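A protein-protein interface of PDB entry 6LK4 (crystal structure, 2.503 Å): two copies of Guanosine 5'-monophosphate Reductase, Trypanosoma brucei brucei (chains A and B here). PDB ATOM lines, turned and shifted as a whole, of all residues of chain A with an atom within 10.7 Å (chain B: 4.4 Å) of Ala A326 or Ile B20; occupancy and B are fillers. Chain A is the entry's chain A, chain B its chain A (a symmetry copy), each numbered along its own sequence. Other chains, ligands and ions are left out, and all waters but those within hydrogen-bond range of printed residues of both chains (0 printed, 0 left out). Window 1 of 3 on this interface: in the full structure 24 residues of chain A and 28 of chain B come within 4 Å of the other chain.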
ATOM      1  N   ILE A   9     -16.457  14.309  -3.379  1.00  0.00           N
ATOM      2  CA  ILE A   9     -17.263  14.051  -2.194  1.00  0.00           C
ATOM      3  C   ILE A   9     -18.527  13.315  -2.642  1.00  0.00           C
ATOM      4  O   ILE A   9     -19.239  13.796  -3.529  1.00  0.00           O
ATOM      5  CB  ILE A   9     -17.555  15.375  -1.464  1.00  0.00           C
ATOM      6  CG1 ILE A   9     -16.255  15.928  -0.886  1.00  0.00           C
ATOM      7  CG2 ILE A   9     -18.586  15.212  -0.379  1.00  0.00           C
ATOM      8  CD1 ILE A   9     -16.376  17.307  -0.310  1.00  0.00           C
ATOM      9  N   PRO A  10     -18.848  12.156  -2.088  1.00  0.00           N
ATOM     10  CA  PRO A  10     -20.052  11.440  -2.534  1.00  0.00           C
ATOM     11  C   PRO A  10     -21.316  12.132  -2.047  1.00  0.00           C
ATOM     12  O   PRO A  10     -21.296  12.983  -1.154  1.00  0.00           O
ATOM     13  CB  PRO A  10     -19.899  10.061  -1.900  1.00  0.00           C
ATOM     14  CG  PRO A  10     -19.115  10.329  -0.640  1.00  0.00           C
ATOM     15  CD  PRO A  10     -18.142  11.441  -1.006  1.00  0.00           C
ATOM     16  N   ALA A 261     -25.720   8.478  20.620  1.00  0.00           N
ATOM     17  CA  ALA A 261     -25.765   9.207  19.358  1.00  0.00           C
ATOM     18  C   ALA A 261     -24.721   8.702  18.372  1.00  0.00           C
ATOM     19  O   ALA A 261     -24.964   8.690  17.158  1.00  0.00           O
ATOM     20  CB  ALA A 261     -25.574  10.697  19.610  1.00  0.00           C
ATOM     21  N   HIS A 262     -23.577   8.245  18.865  1.00  0.00           N
ATOM     22  CA  HIS A 262     -22.471   7.834  18.007  1.00  0.00           C
ATOM     23  C   HIS A 262     -22.124   6.373  18.317  1.00  0.00           C
ATOM     24  O   HIS A 262     -21.200   6.076  19.075  1.00  0.00           O
ATOM     25  CB  HIS A 262     -21.295   8.786  18.219  1.00  0.00           C
ATOM     26  CG  HIS A 262     -20.170   8.585  17.260  1.00  0.00           C
ATOM     27  ND1 HIS A 262     -20.324   7.920  16.062  1.00  0.00           N
ATOM     28  CD2 HIS A 262     -18.867   8.955  17.327  1.00  0.00           C
ATOM     29  CE1 HIS A 262     -19.161   7.882  15.434  1.00  0.00           C
ATOM     30  NE2 HIS A 262     -18.262   8.507  16.178  1.00  0.00           N
ATOM     31  N   GLY A 263     -22.867   5.459  17.694  1.00  0.00           N
ATOM     32  CA  GLY A 263     -22.720   4.037  17.950  1.00  0.00           C
ATOM     33  C   GLY A 263     -21.454   3.407  17.394  1.00  0.00           C
ATOM     34  O   GLY A 263     -21.071   2.322  17.852  1.00  0.00           O
ATOM     35  N   ASN A 290     -26.452   4.447  17.781  1.00  0.00           N
ATOM     36  CA  ASN A 290     -26.859   4.551  16.393  1.00  0.00           C
ATOM     37  C   ASN A 290     -25.695   4.657  15.420  1.00  0.00           C
ATOM     38  O   ASN A 290     -24.670   5.244  15.726  1.00  0.00           O
ATOM     39  CB  ASN A 290     -27.766   5.756  16.224  1.00  0.00           C
ATOM     40  CG  ASN A 290     -29.191   5.466  16.635  1.00  0.00           C
ATOM     41  OD1 ASN A 290     -29.469   4.504  17.370  1.00  0.00           O
ATOM     42  ND2 ASN A 290     -30.115   6.285  16.149  1.00  0.00           N
ATOM     43  N   ILE A 291     -25.892   4.111  14.220  1.00  0.00           N
ATOM     44  CA  ILE A 291     -24.847   4.025  13.217  1.00  0.00           C
ATOM     45  C   ILE A 291     -25.390   4.445  11.860  1.00  0.00           C
ATOM     46  O   ILE A 291     -26.600   4.488  11.623  1.00  0.00           O
ATOM     47  CB  ILE A 291     -24.260   2.603  13.128  1.00  0.00           C
ATOM     48  CG1 ILE A 291     -25.378   1.583  12.922  1.00  0.00           C
ATOM     49  CG2 ILE A 291     -23.505   2.294  14.377  1.00  0.00           C
ATOM     50  CD1 ILE A 291     -24.905   0.283  12.302  1.00  0.00           C
ATOM     51  N   ALA A 292     -24.466   4.728  10.952  1.00  0.00           N
ATOM     52  CA  ALA A 292     -24.835   5.207   9.637  1.00  0.00           C
ATOM     53  C   ALA A 292     -23.929   4.706   8.521  1.00  0.00           C
ATOM     54  O   ALA A 292     -24.144   5.087   7.365  1.00  0.00           O
ATOM     55  CB  ALA A 292     -24.865   6.739   9.634  1.00  0.00           C
ATOM     56  N   SER A 293     -22.970   3.838   8.797  1.00  0.00           N
ATOM     57  CA  SER A 293     -22.041   3.385   7.770  1.00  0.00           C
ATOM     58  C   SER A 293     -21.970   1.865   7.755  1.00  0.00           C
ATOM     59  O   SER A 293     -22.306   1.186   8.729  1.00  0.00           O
ATOM     60  CB  SER A 293     -20.624   3.952   7.986  1.00  0.00           C
ATOM     61  OG  SER A 293     -19.948   3.273   9.039  1.00  0.00           O
ATOM     62  N   GLY A 311     -29.259   5.571  12.039  1.00  0.00           N
ATOM     63  CA  GLY A 311     -29.609   6.983  12.045  1.00  0.00           C
ATOM     64  C   GLY A 311     -28.674   7.852  12.861  1.00  0.00           C
ATOM     65  O   GLY A 311     -28.731   7.834  14.090  1.00  0.00           O
ATOM     66  N   VAL A 312     -27.796   8.598  12.199  1.00  0.00           N
ATOM     67  CA  VAL A 312     -26.942   9.585  12.850  1.00  0.00           C
ATOM     68  C   VAL A 312     -27.172  10.895  12.132  1.00  0.00           C
ATOM     69  O   VAL A 312     -26.772  11.042  10.969  1.00  0.00           O
ATOM     70  CB  VAL A 312     -25.456   9.217  12.805  1.00  0.00           C
ATOM     71  CG1 VAL A 312     -24.639  10.316  13.498  1.00  0.00           C
ATOM     72  CG2 VAL A 312     -25.216   7.848  13.434  1.00  0.00           C
ATOM     73  N   GLY A 313     -27.785  11.856  12.814  1.00  0.00           N
ATOM     74  CA  GLY A 313     -28.169  13.089  12.159  1.00  0.00           C
ATOM     75  C   GLY A 313     -29.135  12.870  11.003  1.00  0.00           C
ATOM     76  O   GLY A 313     -28.943  13.376   9.889  1.00  0.00           O
ATOM     77  N   PRO A 314     -30.213  12.111  11.255  1.00  0.00           N
ATOM     78  CA  PRO A 314     -31.157  11.787  10.179  1.00  0.00           C
ATOM     79  C   PRO A 314     -32.076  12.934   9.784  1.00  0.00           C
ATOM     80  O   PRO A 314     -32.419  13.053   8.607  1.00  0.00           O
ATOM     81  CB  PRO A 314     -31.969  10.625  10.772  1.00  0.00           C
ATOM     82  CG  PRO A 314     -31.252  10.234  12.041  1.00  0.00           C
ATOM     83  CD  PRO A 314     -30.628  11.482  12.516  1.00  0.00           C
ATOM     84  N   GLY A 315     -32.499  13.774  10.729  1.00  0.00           N
ATOM     85  CA  GLY A 315     -33.420  14.852  10.394  1.00  0.00           C
ATOM     86  C   GLY A 315     -32.705  16.079   9.859  1.00  0.00           C
ATOM     87  O   GLY A 315     -31.550  16.354  10.192  1.00  0.00           O
ATOM     88  N   SER A 316     -33.424  16.844   9.029  1.00  0.00           N
ATOM     89  CA  SER A 316     -32.824  18.006   8.370  1.00  0.00           C
ATOM     90  C   SER A 316     -32.345  19.053   9.382  1.00  0.00           C
ATOM     91  O   SER A 316     -31.311  19.699   9.171  1.00  0.00           O
ATOM     92  CB  SER A 316     -33.815  18.617   7.376  1.00  0.00           C
ATOM     93  N   ILE A 317     -33.063  19.227  10.490  1.00  0.00           N
ATOM     94  CA  ILE A 317     -32.670  20.165  11.536  1.00  0.00           C
ATOM     95  C   ILE A 317     -32.695  19.391  12.847  1.00  0.00           C
ATOM     96  O   ILE A 317     -33.757  19.219  13.457  1.00  0.00           O
ATOM     97  CB  ILE A 317     -33.584  21.397  11.601  1.00  0.00           C
ATOM     98  N   CYS A 318     -31.535  18.916  13.283  1.00  0.00           N
ATOM     99  CA  CYS A 318     -31.413  18.187  14.532  1.00  0.00           C
ATOM    100  C   CYS A 318     -30.109  18.595  15.203  1.00  0.00           C
ATOM    101  O   CYS A 318     -29.168  19.044  14.544  1.00  0.00           O
ATOM    102  CB  CYS A 318     -31.441  16.680  14.297  1.00  0.00           C
ATOM    103  SG  CYS A 318     -30.074  16.144  13.260  1.00  0.00           S
ATOM    104  N   ILE A 319     -30.062  18.428  16.526  1.00  0.00           N
ATOM    105  CA  ILE A 319     -28.911  18.882  17.304  1.00  0.00           C
ATOM    106  C   ILE A 319     -27.611  18.387  16.676  1.00  0.00           C
ATOM    107  O   ILE A 319     -26.652  19.150  16.502  1.00  0.00           O
ATOM    108  CB  ILE A 319     -29.045  18.430  18.777  1.00  0.00           C
ATOM    109  N   THR A 320     -27.580  17.121  16.274  1.00  0.00           N
ATOM    110  CA  THR A 320     -26.342  16.538  15.773  1.00  0.00           C
ATOM    111  C   THR A 320     -25.792  17.312  14.582  1.00  0.00           C
ATOM    112  O   THR A 320     -24.584  17.568  14.504  1.00  0.00           O
ATOM    113  CB  THR A 320     -26.592  15.085  15.407  1.00  0.00           C
ATOM    114  OG1 THR A 320     -27.108  14.430  16.562  1.00  0.00           O
ATOM    115  CG2 THR A 320     -25.314  14.404  14.979  1.00  0.00           C
ATOM    116  N   ARG A 321     -26.660  17.703  13.651  1.00  0.00           N
ATOM    117  CA  ARG A 321     -26.191  18.441  12.481  1.00  0.00           C
ATOM    118  C   ARG A 321     -25.812  19.878  12.832  1.00  0.00           C
ATOM    119  O   ARG A 321     -24.794  20.390  12.361  1.00  0.00           O
ATOM    120  CB  ARG A 321     -27.265  18.432  11.400  1.00  0.00           C
ATOM    121  CG  ARG A 321     -27.519  17.084  10.794  1.00  0.00           C
ATOM    122  CD  ARG A 321     -28.348  17.268   9.558  1.00  0.00           C
ATOM    123  NE  ARG A 321     -28.731  15.991   8.971  1.00  0.00           N
ATOM    124  CZ  ARG A 321     -29.423  15.881   7.846  1.00  0.00           C
ATOM    125  NH1 ARG A 321     -29.797  16.972   7.194  1.00  0.00           N
ATOM    126  NH2 ARG A 321     -29.739  14.689   7.377  1.00  0.00           N
ATOM    127  N   LEU A 322     -26.619  20.546  13.650  1.00  0.00           N
ATOM    128  CA  LEU A 322     -26.391  21.959  13.915  1.00  0.00           C
ATOM    129  C   LEU A 322     -25.245  22.176  14.884  1.00  0.00           C
ATOM    130  O   LEU A 322     -24.515  23.167  14.763  1.00  0.00           O
ATOM    131  CB  LEU A 322     -27.662  22.601  14.469  1.00  0.00           C
ATOM    132  CG  LEU A 322     -28.838  22.642  13.499  1.00  0.00           C
ATOM    133  CD1 LEU A 322     -29.784  23.749  13.890  1.00  0.00           C
ATOM    134  CD2 LEU A 322     -28.346  22.826  12.050  1.00  0.00           C
ATOM    135  N   VAL A 323     -25.075  21.279  15.849  1.00  0.00           N
ATOM    136  CA  VAL A 323     -24.026  21.459  16.842  1.00  0.00           C
ATOM    137  C   VAL A 323     -22.714  20.862  16.367  1.00  0.00           C
ATOM    138  O   VAL A 323     -21.688  21.550  16.345  1.00  0.00           O
ATOM    139  CB  VAL A 323     -24.455  20.872  18.203  1.00  0.00           C
ATOM    140  CG1 VAL A 323     -23.310  20.914  19.171  1.00  0.00           C
ATOM    141  CG2 VAL A 323     -25.601  21.654  18.769  1.00  0.00           C
ATOM    142  N   ALA A 324     -22.721  19.588  15.959  1.00  0.00           N
ATOM    143  CA  ALA A 324     -21.477  18.931  15.557  1.00  0.00           C
ATOM    144  C   ALA A 324     -21.188  19.008  14.064  1.00  0.00           C
ATOM    145  O   ALA A 324     -20.030  18.838  13.677  1.00  0.00           O
ATOM    146  CB  ALA A 324     -21.476  17.455  15.970  1.00  0.00           C
ATOM    147  N   GLY A 325     -22.197  19.244  13.223  1.00  0.00           N
ATOM    148  CA  GLY A 325     -22.023  19.204  11.781  1.00  0.00           C
ATOM    149  C   GLY A 325     -21.928  17.819  11.190  1.00  0.00           C
ATOM    150  O   GLY A 325     -21.385  17.661  10.090  1.00  0.00           O
ATOM    151  N   ALA A 326     -22.424  16.798  11.889  1.00  0.00           N
ATOM    152  CA  ALA A 326     -22.262  15.418  11.453  1.00  0.00           C
ATOM    153  C   ALA A 326     -23.613  14.812  11.101  1.00  0.00           C
ATOM    154  O   ALA A 326     -24.664  15.270  11.556  1.00  0.00           O
ATOM    155  CB  ALA A 326     -21.592  14.566  12.537  1.00  0.00           C
ATOM    156  N   GLY A 327     -23.574  13.763  10.304  1.00  0.00           N
ATOM    157  CA  GLY A 327     -24.781  13.032   9.973  1.00  0.00           C
ATOM    158  C   GLY A 327     -24.672  12.408   8.601  1.00  0.00           C
ATOM    159  O   GLY A 327     -23.749  12.677   7.836  1.00  0.00           O
ATOM    160  N   VAL A 328     -25.633  11.539   8.309  1.00  0.00           N
ATOM    161  CA  VAL A 328     -25.722  10.901   6.999  1.00  0.00           C
ATOM    162  C   VAL A 328     -27.164  11.019   6.533  1.00  0.00           C
ATOM    163  O   VAL A 328     -28.083  10.774   7.324  1.00  0.00           O
ATOM    164  CB  VAL A 328     -25.278   9.432   7.045  1.00  0.00           C
ATOM    165  CG1 VAL A 328     -25.463   8.784   5.687  1.00  0.00           C
ATOM    166  CG2 VAL A 328     -23.840   9.335   7.472  1.00  0.00           C
ATOM    167  N   PRO A 329     -27.418  11.446   5.300  1.00  0.00           N
ATOM    168  CA  PRO A 329     -28.782  11.370   4.782  1.00  0.00           C
ATOM    169  C   PRO A 329     -29.307   9.950   4.915  1.00  0.00           C
ATOM    170  O   PRO A 329     -28.629   8.982   4.565  1.00  0.00           O
ATOM    171  CB  PRO A 329     -28.628  11.820   3.331  1.00  0.00           C
ATOM    172  CG  PRO A 329     -27.464  12.769   3.388  1.00  0.00           C
ATOM    173  CD  PRO A 329     -26.518  12.161   4.379  1.00  0.00           C
ATOM    174  N   GLN A 330     -30.531   9.843   5.443  1.00  0.00           N
ATOM    175  CA  GLN A 330     -30.995   8.600   6.055  1.00  0.00           C
ATOM    176  C   GLN A 330     -31.216   7.466   5.052  1.00  0.00           C
ATOM    177  O   GLN A 330     -31.105   6.293   5.430  1.00  0.00           O
ATOM    178  CB  GLN A 330     -32.273   8.859   6.843  1.00  0.00           C
ATOM    179  CG  GLN A 330     -32.858   7.647   7.507  1.00  0.00           C
ATOM    180  CD  GLN A 330     -32.037   7.132   8.688  1.00  0.00           C
ATOM    181  OE1 GLN A 330     -30.818   7.310   8.755  1.00  0.00           O
ATOM    182  NE2 GLN A 330     -32.713   6.483   9.631  1.00  0.00           N
ATOM    183  N   ALA A 333     -27.897   5.947   4.407  1.00  0.00           N
ATOM    184  CA  ALA A 333     -27.473   5.240   5.612  1.00  0.00           C
ATOM    185  C   ALA A 333     -28.194   3.897   5.742  1.00  0.00           C
ATOM    186  O   ALA A 333     -27.580   2.874   6.078  1.00  0.00           O
ATOM    187  CB  ALA A 333     -27.711   6.113   6.846  1.00  0.00           C
ATOM    188  N   LEU B  19     -22.104  17.155   5.259  1.00  0.00           N
ATOM    189  CA  LEU B  19     -22.125  16.740   6.652  1.00  0.00           C
ATOM    190  C   LEU B  19     -20.857  15.946   6.936  1.00  0.00           C
ATOM    191  O   LEU B  19     -20.303  15.301   6.042  1.00  0.00           O
ATOM    192  CB  LEU B  19     -23.353  15.887   6.980  1.00  0.00           C
ATOM    193  CG  LEU B  19     -24.765  16.489   6.920  1.00  0.00           C
ATOM    194  CD1 LEU B  19     -25.811  15.408   7.198  1.00  0.00           C
ATOM    195  CD2 LEU B  19     -24.907  17.593   7.920  1.00  0.00           C
ATOM    196  N   ILE B  20     -20.371  16.031   8.172  1.00  0.00           N
ATOM    197  CA  ILE B  20     -19.247  15.196   8.570  1.00  0.00           C
ATOM    198  C   ILE B  20     -19.721  13.754   8.710  1.00  0.00           C
ATOM    199  O   ILE B  20     -20.697  13.475   9.417  1.00  0.00           O
ATOM    200  CB  ILE B  20     -18.629  15.722   9.873  1.00  0.00           C
ATOM    201  CG1 ILE B  20     -17.880  17.027   9.600  1.00  0.00           C
ATOM    202  CG2 ILE B  20     -17.679  14.677  10.498  1.00  0.00           C
ATOM    203  CD1 ILE B  20     -17.528  17.802  10.855  1.00  0.00           C
ATOM    204  N   ILE B  21     -19.042  12.830   8.043  1.00  0.00           N
ATOM    205  CA  ILE B  21     -19.443  11.423   8.132  1.00  0.00           C
ATOM    206  C   ILE B  21     -18.954  10.848   9.458  1.00  0.00           C
ATOM    207  O   ILE B  21     -17.766  10.996   9.783  1.00  0.00           O
ATOM    208  CB  ILE B  21     -18.898  10.615   6.967  1.00  0.00           C
ATOM    209  CG1 ILE B  21     -19.454  11.116   5.623  1.00  0.00           C
ATOM    210  CG2 ILE B  21     -19.255   9.164   7.203  1.00  0.00           C
ATOM    211  CD1 ILE B  21     -18.954  10.314   4.439  1.00  0.00           C
ATOM    212  N   PRO B  22     -19.810  10.182  10.230  1.00  0.00           N
ATOM    213  CA  PRO B  22     -19.358   9.593  11.499  1.00  0.00           C
ATOM    214  C   PRO B  22     -18.350   8.486  11.265  1.00  0.00           C
ATOM    215  O   PRO B  22     -18.570   7.588  10.453  1.00  0.00           O
ATOM    216  CB  PRO B  22     -20.647   9.064  12.120  1.00  0.00           C
ATOM    217  CG  PRO B  22     -21.697   9.919  11.534  1.00  0.00           C
ATOM    218  CD  PRO B  22     -21.270  10.129  10.101  1.00  0.00           C
ATOM    219  N   SER B 361     -16.890  22.867  12.821  1.00  0.00           N
ATOM    220  CA  SER B 361     -16.320  21.526  12.689  1.00  0.00           C
ATOM    221  C   SER B 361     -16.035  21.178  11.246  1.00  0.00           C
ATOM    222  O   SER B 361     -15.070  20.461  10.963  1.00  0.00           O
ATOM    223  CB  SER B 361     -17.246  20.457  13.277  1.00  0.00           C
ATOM    224  OG  SER B 361     -17.807  20.855  14.508  1.00  0.00           O
ATOM    225  N   LYS B 362     -16.878  21.644  10.327  1.00  0.00           N
ATOM    226  CA  LYS B 362     -16.631  21.377   8.916  1.00  0.00           C
ATOM    227  C   LYS B 362     -15.440  22.184   8.424  1.00  0.00           C
ATOM    228  O   LYS B 362     -14.610  21.682   7.659  1.00  0.00           O
ATOM    229  CB  LYS B 362     -17.879  21.696   8.084  1.00  0.00           C
ATOM    230  CG  LYS B 362     -19.144  21.031   8.587  1.00  0.00           C
ATOM    231  CD  LYS B 362     -20.370  21.537   7.864  1.00  0.00           C
ATOM    232  CE  LYS B 362     -21.643  20.888   8.405  1.00  0.00           C
ATOM    233  NZ  LYS B 362     -22.830  21.374   7.647  1.00  0.00           N
ATOM    234  N   TYR B 457     -17.028  12.834  16.413  1.00  0.00           N
ATOM    235  CA  TYR B 457     -17.674  12.135  15.308  1.00  0.00           C
ATOM    236  C   TYR B 457     -16.673  11.728  14.229  1.00  0.00           C
ATOM    237  O   TYR B 457     -16.868  10.704  13.560  1.00  0.00           O
ATOM    238  CB  TYR B 457     -18.792  12.996  14.722  1.00  0.00           C
ATOM    239  CG  TYR B 457     -20.121  12.818  15.450  1.00  0.00           C
ATOM    240  CD1 TYR B 457     -20.886  11.673  15.256  1.00  0.00           C
ATOM    241  CD2 TYR B 457     -20.601  13.796  16.339  1.00  0.00           C
ATOM    242  CE1 TYR B 457     -22.095  11.497  15.911  1.00  0.00           C
ATOM    243  CE2 TYR B 457     -21.808  13.631  17.005  1.00  0.00           C
ATOM    244  CZ  TYR B 457     -22.550  12.473  16.786  1.00  0.00           C
ATOM    245  OH  TYR B 457     -23.754  12.282  17.426  1.00  0.00           O
ATOM    246  N   SER B 458     -15.603  12.505  14.031  1.00  0.00           N
ATOM    247  CA  SER B 458     -14.513  12.055  13.170  1.00  0.00           C
ATOM    248  C   SER B 458     -13.505  11.174  13.908  1.00  0.00           C
ATOM    249  O   SER B 458     -12.487  10.793  13.314  1.00  0.00           O
ATOM    250  CB  SER B 458     -13.787  13.259  12.555  1.00  0.00           C
ATOM    251  OG  SER B 458     -14.644  14.015  11.721  1.00  0.00           O
ATOM    252  N   MET B 466      -8.414  15.834  13.265  1.00  0.00           N
ATOM    253  CA  MET B 466      -9.653  16.298  12.659  1.00  0.00           C
ATOM    254  C   MET B 466      -9.458  16.627  11.182  1.00  0.00           C
ATOM    255  O   MET B 466     -10.312  16.310  10.345  1.00  0.00           O
ATOM    256  CB  MET B 466     -10.163  17.514  13.422  1.00  0.00           C
ATOM    257  CG  MET B 466     -11.515  17.984  12.969  1.00  0.00           C
ATOM    258  SD  MET B 466     -12.739  16.691  13.147  1.00  0.00           S
ATOM    259  CE  MET B 466     -14.237  17.644  12.875  1.00  0.00           C
ATOM    260  N   THR B 470     -11.397  13.649   8.810  1.00  0.00           N
ATOM    261  CA  THR B 470     -12.788  13.944   8.506  1.00  0.00           C
ATOM    262  C   THR B 470     -13.115  13.571   7.067  1.00  0.00           C
ATOM    263  O   THR B 470     -12.284  13.700   6.169  1.00  0.00           O
ATOM    264  CB  THR B 470     -13.087  15.414   8.770  1.00  0.00           C
ATOM    265  OG1 THR B 470     -13.110  15.624  10.186  1.00  0.00           O
ATOM    266  CG2 THR B 470     -14.436  15.821   8.167  1.00  0.00           C
ATOM    267  N   ARG B 471     -14.309  13.020   6.872  1.00  0.00           N
ATOM    268  CA  ARG B 471     -14.829  12.725   5.555  1.00  0.00           C
ATOM    269  C   ARG B 471     -16.198  13.359   5.463  1.00  0.00           C
ATOM    270  O   ARG B 471     -16.976  13.319   6.422  1.00  0.00           O
ATOM    271  CB  ARG B 471     -14.945  11.235   5.295  1.00  0.00           C
ATOM    272  CG  ARG B 471     -13.635  10.482   5.309  1.00  0.00           C
ATOM    273  CD  ARG B 471     -12.717  10.928   4.193  1.00  0.00           C
ATOM    274  NE  ARG B 471     -11.477  10.139   4.170  1.00  0.00           N
ATOM    275  CZ  ARG B 471     -10.367  10.463   4.835  1.00  0.00           C
ATOM    276  NH1 ARG B 471     -10.330  11.567   5.583  1.00  0.00           N
ATOM    277  NH2 ARG B 471      -9.293   9.685   4.753  1.00  0.00           N
ATOM    278  N   PHE B 472     -16.486  13.939   4.313  1.00  0.00           N
ATOM    279  CA  PHE B 472     -17.740  14.627   4.081  1.00  0.00           C
ATOM    280  C   PHE B 472     -18.675  13.774   3.243  1.00  0.00           C
ATOM    281  O   PHE B 472     -18.238  12.933   2.455  1.00  0.00           O
ATOM    282  CB  PHE B 472     -17.489  15.955   3.370  1.00  0.00           C
ATOM    283  CG  PHE B 472     -16.811  16.962   4.230  1.00  0.00           C
ATOM    284  CD1 PHE B 472     -17.457  17.485   5.334  1.00  0.00           C
ATOM    285  CD2 PHE B 472     -15.522  17.377   3.950  1.00  0.00           C
ATOM    286  CE1 PHE B 472     -16.831  18.415   6.132  1.00  0.00           C
ATOM    287  CE2 PHE B 472     -14.892  18.302   4.749  1.00  0.00           C
ATOM    288  CZ  PHE B 472     -15.547  18.825   5.838  1.00  0.00           C
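No position is printed for both chains.
Of the 20 pairs that touch across the chains among the printed residues, none has its exchanged pair printed and touching as well.
Hydrophobic or aromatic side chains of chain B within 4 Å of the printed part of chain A: Leu B19, Ile B20, Pro B22, Tyr B457 and Phe B472.
Along chain B the printed residues that touch a printed residue of chain A span positions 19 to 472.
Hydrophobic or aromatic side chains of chain A that line the printed part of chain B: Ile A9, Pro A10, Ala A261, His A262, Val A312, Ala A324, Ala A326 and Val A328.
Among the printed residues, 20 pairs touch across the chains.
Printed residues of chain B within 4 Å of Ala A261: Tyr B457.
Printed residues of chain B within 4 Å of His A262: Pro B22 (3.8 Å) and Tyr B457 (3.6 Å).
Val A323 touches none of the printed residues of chain B.
Of the printed residues of chain B, Ala A324 touches Ile B20, Ser B361 and Tyr B457.
Printed residues of chain B within 4 Å of Gly A325: Leu B19 (3.6 Å), Ile B20 (2.7 Å) and Lys B362 (3.6 Å).
Of chain B, only Ile B20 and Tyr B457 come within 4 Å of Ala A326.
Of the printed residues of chain B, Val A328 touches Pro B22.
Ile B20 touches just these residues of chain A: Ala A324 (3.9 Å), Gly A325 (2.7 Å), Ala A326 (3.2 Å) and Gly A327 (3.0 Å).
No residue of chain A comes within 4 Å of Ile B21.
Of chain A, only His A262, Val A312 and Val A328 come within 4 Å of Pro B22.
Lys B362 touches just one residue of chain A: Gly A325 (3.6 Å).
Printed residues of chain A within 4 Å of Tyr B457: Ala A261 (3.3 Å), His A262 (3.6 Å), Val A312 (3.7 Å), Thr A320 (3.6 Å), Ala A324 (3.8 Å) and Ala A326 (3.7 Å).
Phe B472 touches just these residues of chain A: Ile A9 (3.7 Å) and Pro A10 (3.8 Å).
The nearest residue of chain B that does not touch Ala A326 is Leu B19 (4.3 Å).
The nearest residue of chain A that does not touch Ile B20 is Val A328 (5.4 Å).
N of Gly A325 sits at hydrogen-bond distance from O of Thr A320 (3.2 Å).
The backbone NH (N) of Val A328 lies within hydrogen-bond range of the backbone carbonyl oxygen (O) of Val A312.
The backbone NH (N) of Ala A326 is in hydrogen-bond range of the backbone carbonyl oxygen (O) of Thr A320 (3.5 Å).
The guanidinium group (NE) of Arg A321 is in hydrogen-bond range of the backbone carbonyl oxygen (O) of Gly A315 (3.1 Å).
O of Gly A313 is in hydrogen-bond range of NE of Arg A321, 2.8 Å away.
The backbone carbonyl oxygen (O) of Pro A314 sits at hydrogen-bond distance from the guanidinium group (NH2) of Arg A321 (3.4 Å).
Phe B472 touches Pro A10.
Ala A261 touches Tyr B457 (CB to OH, 3.3 Å).
CG of Pro B22 touches CG1 of Val A312, 3.6 Å away.
Thr A320 touches Tyr B457.
Arg A321 touches Leu B19 (NE to CD1, 3.5 Å).
CD2 of Tyr B457 touches CB of Ala A324, at 3.8 Å.
Lys B362 touches Gly A325.
CG of Tyr B457 touches CB of Ala A326, 3.7 Å away.
CB of Leu B19 touches O of Gly A327 (3.3 Å).
CG2 of Val A328 touches CD of Pro B22, 3.8 Å away.
O of Ala A324 sits at hydrogen-bond distance from OG of Ser B361, 3.1 Å away.
The backbone NH (N) of Gly A327 lies within hydrogen-bond range of the backbone carbonyl oxygen (O) of Ile B20, at 3.0 Å.
The backbone NH (N) of Ile B20 lies within hydrogen-bond range of the backbone carbonyl oxygen (O) of Gly A325 (2.7 Å).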
